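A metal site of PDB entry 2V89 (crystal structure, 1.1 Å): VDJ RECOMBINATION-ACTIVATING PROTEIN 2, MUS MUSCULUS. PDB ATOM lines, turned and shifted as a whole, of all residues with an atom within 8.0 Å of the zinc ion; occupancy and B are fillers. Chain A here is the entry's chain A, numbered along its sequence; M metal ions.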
ATOM      1  N   CYS A  14     -21.169  -1.901  -7.138  1.00  0.00           N
ATOM      2  CA  CYS A  14     -20.350  -1.425  -6.027  1.00  0.00           C
ATOM      3  C   CYS A  14     -20.561   0.010  -5.643  1.00  0.00           C
ATOM      4  O   CYS A  14     -20.188   0.461  -4.554  1.00  0.00           O
ATOM      5  CB  CYS A  14     -18.867  -1.700  -6.304  1.00  0.00           C
ATOM      6  SG  CYS A  14     -18.029  -0.497  -7.424  1.00  0.00           S
ATOM      7  N   CYS A  15     -21.151   0.815  -6.522  1.00  0.00           N
ATOM      8  CA  CYS A  15     -21.357   2.243  -6.371  1.00  0.00           C
ATOM      9  C   CYS A  15     -22.407   2.677  -7.411  1.00  0.00           C
ATOM     10  O   CYS A  15     -22.740   1.888  -8.308  1.00  0.00           O
ATOM     11  CB  CYS A  15     -20.066   3.005  -6.493  1.00  0.00           C
ATOM     12  SG  CYS A  15     -19.362   3.030  -8.153  1.00  0.00           S
ATOM     13  N   ILE A  39     -10.987  -3.013  -3.853  1.00  0.00           N
ATOM     14  CA  ILE A  39     -10.331  -2.319  -2.737  1.00  0.00           C
ATOM     15  C   ILE A  39     -11.386  -2.034  -1.671  1.00  0.00           C
ATOM     16  O   ILE A  39     -12.531  -1.748  -1.943  1.00  0.00           O
ATOM     17  CB  ILE A  39      -9.553  -1.083  -3.208  1.00  0.00           C
ATOM     18  CG1 ILE A  39      -8.733  -0.406  -2.075  1.00  0.00           C
ATOM     19  CG2 ILE A  39     -10.424  -0.098  -3.928  1.00  0.00           C
ATOM     20  CD1 ILE A  39      -7.695   0.574  -2.574  1.00  0.00           C
ATOM     21  N   TYR A  40     -10.903  -2.094  -0.415  1.00  0.00           N
ATOM     22  CA  TYR A  40     -11.785  -1.901   0.738  1.00  0.00           C
ATOM     23  C   TYR A  40     -11.838  -0.452   1.170  1.00  0.00           C
ATOM     24  O   TYR A  40     -10.808   0.166   1.456  1.00  0.00           O
ATOM     25  CB  TYR A  40     -11.229  -2.749   1.909  1.00  0.00           C
ATOM     26  CG  TYR A  40     -12.100  -2.716   3.121  1.00  0.00           C
ATOM     27  CD1 TYR A  40     -13.353  -3.313   3.107  1.00  0.00           C
ATOM     28  CD2 TYR A  40     -11.698  -2.071   4.273  1.00  0.00           C
ATOM     29  CE1 TYR A  40     -14.132  -3.255   4.218  1.00  0.00           C
ATOM     30  CE2 TYR A  40     -12.491  -2.028   5.408  1.00  0.00           C
ATOM     31  CZ  TYR A  40     -13.725  -2.635   5.382  1.00  0.00           C
ATOM     32  OH  TYR A  40     -14.550  -2.621   6.484  1.00  0.00           O
ATOM     33  N   CYS A  41     -13.043   0.082   1.279  1.00  0.00           N
ATOM     34  CA  CYS A  41     -13.307   1.432   1.808  1.00  0.00           C
ATOM     35  C   CYS A  41     -13.703   1.322   3.263  1.00  0.00           C
ATOM     36  O   CYS A  41     -14.609   0.548   3.622  1.00  0.00           O
ATOM     37  CB  CYS A  41     -14.397   2.066   0.956  1.00  0.00           C
ATOM     38  SG  CYS A  41     -14.938   3.669   1.661  1.00  0.00           S
ATOM     39  N   SER A  42     -13.058   2.161   4.071  1.00  0.00           N
ATOM     40  CA  SER A  42     -13.252   2.165   5.519  1.00  0.00           C
ATOM     41  C   SER A  42     -14.425   3.017   6.001  1.00  0.00           C
ATOM     42  O   SER A  42     -14.642   3.112   7.231  1.00  0.00           O
ATOM     43  CB  SER A  42     -11.966   2.590   6.214  1.00  0.00           C
ATOM     44  OG  SER A  42     -10.942   1.616   6.056  1.00  0.00           O
ATOM     45  N   HIS A  43     -15.206   3.591   5.130  1.00  0.00           N
ATOM     46  CA  HIS A  43     -16.361   4.376   5.548  1.00  0.00           C
ATOM     47  C   HIS A  43     -17.387   3.555   6.277  1.00  0.00           C
ATOM     48  O   HIS A  43     -17.803   2.497   5.820  1.00  0.00           O
ATOM     49  CB  HIS A  43     -17.058   5.020   4.355  1.00  0.00           C
ATOM     50  CG  HIS A  43     -18.307   5.735   4.663  1.00  0.00           C
ATOM     51  ND1 HIS A  43     -18.271   6.970   5.229  1.00  0.00           N
ATOM     52  CD2 HIS A  43     -19.585   5.370   4.510  1.00  0.00           C
ATOM     53  CE1 HIS A  43     -19.525   7.348   5.378  1.00  0.00           C
ATOM     54  NE2 HIS A  43     -20.361   6.423   4.971  1.00  0.00           N
ATOM     55  N   GLY A  44     -17.841   4.023   7.418  1.00  0.00           N
ATOM     56  CA  GLY A  44     -18.976   3.385   8.107  1.00  0.00           C
ATOM     57  C   GLY A  44     -18.637   2.005   8.560  1.00  0.00           C
ATOM     58  O   GLY A  44     -17.583   1.789   9.188  1.00  0.00           O
ATOM     59  N   GLY A  46     -17.931  -0.245   6.453  1.00  0.00           N
ATOM     60  CA  GLY A  46     -17.002  -0.673   5.421  1.00  0.00           C
ATOM     61  C   GLY A  46     -17.757  -1.225   4.225  1.00  0.00           C
ATOM     62  O   GLY A  46     -18.880  -1.706   4.320  1.00  0.00           O
ATOM     63  N   HIS A  47     -17.065  -1.219   3.084  1.00  0.00           N
ATOM     64  CA  HIS A  47     -17.579  -1.885   1.884  1.00  0.00           C
ATOM     65  C   HIS A  47     -16.455  -2.023   0.883  1.00  0.00           C
ATOM     66  O   HIS A  47     -15.431  -1.367   0.998  1.00  0.00           O
ATOM     67  CB  HIS A  47     -18.792  -1.148   1.299  1.00  0.00           C
ATOM     68  CG  HIS A  47     -18.437   0.200   0.714  1.00  0.00           C
ATOM     69  ND1 HIS A  47     -18.690   0.503  -0.591  1.00  0.00           N
ATOM     70  CD2 HIS A  47     -17.867   1.331   1.213  1.00  0.00           C
ATOM     71  CE1 HIS A  47     -18.293   1.747  -0.840  1.00  0.00           C
ATOM     72  NE2 HIS A  47     -17.746   2.293   0.226  1.00  0.00           N
ATOM     73  N   TRP A  48     -16.669  -2.882  -0.109  1.00  0.00           N
ATOM     74  CA  TRP A  48     -15.695  -3.125  -1.170  1.00  0.00           C
ATOM     75  C   TRP A  48     -16.133  -2.504  -2.481  1.00  0.00           C
ATOM     76  O   TRP A  48     -17.314  -2.585  -2.829  1.00  0.00           O
ATOM     77  CB  TRP A  48     -15.452  -4.631  -1.397  1.00  0.00           C
ATOM     78  CG  TRP A  48     -14.768  -5.314  -0.249  1.00  0.00           C
ATOM     79  CD1 TRP A  48     -15.327  -5.801   0.929  1.00  0.00           C
ATOM     80  CD2 TRP A  48     -13.389  -5.599  -0.170  1.00  0.00           C
ATOM     81  NE1 TRP A  48     -14.347  -6.358   1.704  1.00  0.00           N
ATOM     82  CE2 TRP A  48     -13.128  -6.247   1.058  1.00  0.00           C
ATOM     83  CE3 TRP A  48     -12.318  -5.346  -1.044  1.00  0.00           C
ATOM     84  CZ2 TRP A  48     -11.838  -6.662   1.436  1.00  0.00           C
ATOM     85  CZ3 TRP A  48     -11.054  -5.733  -0.697  1.00  0.00           C
ATOM     86  CH2 TRP A  48     -10.838  -6.377   0.507  1.00  0.00           C
ATOM     87  N   VAL A  49     -15.188  -1.903  -3.207  1.00  0.00           N
ATOM     88  CA  VAL A  49     -15.464  -1.332  -4.507  1.00  0.00           C
ATOM     89  C   VAL A  49     -14.510  -1.926  -5.529  1.00  0.00           C
ATOM     90  O   VAL A  49     -13.397  -2.332  -5.230  1.00  0.00           O
ATOM     91  CB  VAL A  49     -15.382   0.207  -4.508  1.00  0.00           C
ATOM     92  CG1 VAL A  49     -16.505   0.803  -3.681  1.00  0.00           C
ATOM     93  CG2 VAL A  49     -14.021   0.724  -4.002  1.00  0.00           C
ATOM     94  N   MET A  54     -13.471   2.994  -9.414  1.00  0.00           N
ATOM     95  CA  MET A  54     -12.870   4.168  -8.771  1.00  0.00           C
ATOM     96  C   MET A  54     -11.881   4.886  -9.668  1.00  0.00           C
ATOM     97  O   MET A  54     -11.224   5.847  -9.212  1.00  0.00           O
ATOM     98  CB  MET A  54     -12.166   3.742  -7.472  1.00  0.00           C
ATOM     99  CG  MET A  54     -13.074   3.110  -6.459  1.00  0.00           C
ATOM    100  SD  MET A  54     -14.461   4.102  -5.913  1.00  0.00           S
ATOM    101  CE  MET A  54     -15.840   3.352  -6.805  1.00  0.00           C
ATOM    102  N   TYR A  71      -8.144   3.200   3.029  1.00  0.00           N
ATOM    103  CA  TYR A  71      -8.658   3.818   1.826  1.00  0.00           C
ATOM    104  C   TYR A  71     -10.114   4.236   2.042  1.00  0.00           C
ATOM    105  O   TYR A  71     -10.888   3.482   2.642  1.00  0.00           O
ATOM    106  CB  TYR A  71      -8.581   2.837   0.642  1.00  0.00           C
ATOM    107  CG  TYR A  71      -9.161   3.279  -0.622  1.00  0.00           C
ATOM    108  CD1 TYR A  71     -10.431   2.811  -1.029  1.00  0.00           C
ATOM    109  CD2 TYR A  71      -8.523   4.209  -1.450  1.00  0.00           C
ATOM    110  CE1 TYR A  71     -10.969   3.235  -2.214  1.00  0.00           C
ATOM    111  CE2 TYR A  71      -9.109   4.637  -2.623  1.00  0.00           C
ATOM    112  CZ  TYR A  71     -10.323   4.144  -3.022  1.00  0.00           C
ATOM    113  OH  TYR A  71     -10.969   4.564  -4.171  1.00  0.00           O
ATOM    114  N   TYR A  72     -10.468   5.392   1.525  1.00  0.00           N
ATOM    115  CA  TYR A  72     -11.831   5.858   1.402  1.00  0.00           C
ATOM    116  C   TYR A  72     -12.143   6.096  -0.085  1.00  0.00           C
ATOM    117  O   TYR A  72     -11.376   6.745  -0.804  1.00  0.00           O
ATOM    118  CB  TYR A  72     -12.046   7.156   2.203  1.00  0.00           C
ATOM    119  CG  TYR A  72     -11.879   6.893   3.678  1.00  0.00           C
ATOM    120  CD1 TYR A  72     -10.666   6.939   4.340  1.00  0.00           C
ATOM    121  CD2 TYR A  72     -13.014   6.571   4.399  1.00  0.00           C
ATOM    122  CE1 TYR A  72     -10.613   6.678   5.698  1.00  0.00           C
ATOM    123  CE2 TYR A  72     -12.967   6.287   5.759  1.00  0.00           C
ATOM    124  CZ  TYR A  72     -11.751   6.335   6.408  1.00  0.00           C
ATOM    125  OH  TYR A  72     -11.574   6.082   7.734  1.00  0.00           O
ATOM    126  N   CYS A  73     -13.262   5.524  -0.520  1.00  0.00           N
ATOM    127  CA  CYS A  73     -13.647   5.611  -1.927  1.00  0.00           C
ATOM    128  C   CYS A  73     -14.120   6.986  -2.334  1.00  0.00           C
ATOM    129  O   CYS A  73     -14.308   7.892  -1.534  1.00  0.00           O
ATOM    130  CB  CYS A  73     -14.711   4.551  -2.225  1.00  0.00           C
ATOM    131  SG  CYS A  73     -16.379   5.028  -1.679  1.00  0.00           S
ATOM    132  N   ASN A  74     -14.345   7.111  -3.659  1.00  0.00           N
ATOM    133  CA  ASN A  74     -14.750   8.395  -4.204  1.00  0.00           C
ATOM    134  C   ASN A  74     -16.043   8.946  -3.688  1.00  0.00           C
ATOM    135  O   ASN A  74     -16.210  10.170  -3.617  1.00  0.00           O
ATOM    136  CB  ASN A  74     -14.794   8.349  -5.743  1.00  0.00           C
ATOM    137  CG  ASN A  74     -13.528   7.985  -6.456  1.00  0.00           C
ATOM    138  OD1 ASN A  74     -13.518   7.512  -7.631  1.00  0.00           O
ATOM    139  ND2 ASN A  74     -12.394   8.155  -5.836  1.00  0.00           N
ATOM    140  N   GLU A  75     -16.984   8.131  -3.284  1.00  0.00           N
ATOM    141  CA  GLU A  75     -18.254   8.522  -2.714  1.00  0.00           C
ATOM    142  C   GLU A  75     -18.073   8.998  -1.259  1.00  0.00           C
ATOM    143  O   GLU A  75     -18.969   9.772  -0.870  1.00  0.00           O
ATOM    144  CB  GLU A  75     -19.273   7.386  -2.620  1.00  0.00           C
ATOM    145  CG  GLU A  75     -20.104   7.127  -3.854  1.00  0.00           C
ATOM    146  CD  GLU A  75     -21.058   5.995  -3.477  1.00  0.00           C
ATOM    147  OE1 GLU A  75     -20.623   4.851  -3.605  1.00  0.00           O
ATOM    148  OE2 GLU A  75     -22.186   6.337  -3.067  1.00  0.00           O
ATOM    149  N   HIS A  76     -17.100   8.510  -0.519  1.00  0.00           N
ATOM    150  CA  HIS A  76     -17.090   8.715   0.934  1.00  0.00           C
ATOM    151  C   HIS A  76     -15.925   9.552   1.424  1.00  0.00           C
ATOM    152  O   HIS A  76     -15.994   9.980   2.595  1.00  0.00           O
ATOM    153  CB  HIS A  76     -17.092   7.335   1.659  1.00  0.00           C
ATOM    154  CG  HIS A  76     -18.357   6.563   1.413  1.00  0.00           C
ATOM    155  ND1 HIS A  76     -18.319   5.222   1.081  1.00  0.00           N
ATOM    156  CD2 HIS A  76     -19.628   6.974   1.491  1.00  0.00           C
ATOM    157  CE1 HIS A  76     -19.584   4.845   0.965  1.00  0.00           C
ATOM    158  NE2 HIS A  76     -20.407   5.855   1.169  1.00  0.00           N
ATOM    159  N   VAL A  77     -14.858   9.727   0.639  1.00  0.00           N
ATOM    160  CA  VAL A  77     -13.653  10.389   1.163  1.00  0.00           C
ATOM    161  C   VAL A  77     -13.917  11.819   1.543  1.00  0.00           C
ATOM    162  O   VAL A  77     -13.262  12.338   2.459  1.00  0.00           O
ATOM    163  CB  VAL A  77     -12.502  10.220   0.171  1.00  0.00           C
ATOM    164  CG1 VAL A  77     -12.727  10.952  -1.161  1.00  0.00           C
ATOM    165  CG2 VAL A  77     -11.199  10.693   0.811  1.00  0.00           C
ATOM    166  N   ILE A  79     -16.519  12.988   3.157  1.00  0.00           N
ATOM    167  CA  ILE A  79     -17.393  13.123   4.303  1.00  0.00           C
ATOM    168  C   ILE A  79     -16.548  13.304   5.552  1.00  0.00           C
ATOM    169  O   ILE A  79     -15.614  12.544   5.814  1.00  0.00           O
ATOM    170  CB  ILE A  79     -18.247  11.848   4.455  1.00  0.00           C
ATOM    171  CG1 ILE A  79     -19.055  11.615   3.199  1.00  0.00           C
ATOM    172  CG2 ILE A  79     -19.033  11.905   5.768  1.00  0.00           C
ATOM    173  CD1 ILE A  79     -19.932  10.377   3.220  1.00  0.00           C
HETATM  174 ZN    ZN M   1     -16.805   4.064   0.383  1.00  0.00          ZN
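Of the 21 residues printed, 4 come within 4 Å of the zinc ion.
The zinc ion is bound by a ring nitrogen (NE2) of His 47. The zinc ion is bound by ND1 of His 76 (2.0 Å). The zinc ion is bound by SG of Cys 41 (2.3 Å). The zinc ion is bound by the side-chain sulfur (SG) of Cys 73.
The side-chain sulfur (SG) of Cys 41 sits close to the backbone NH (N) of His 43 (3.5 Å). The side-chain sulfur (SG) of Cys 73 lies close to the backbone NH (N) of Glu 75 (3.5 Å).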
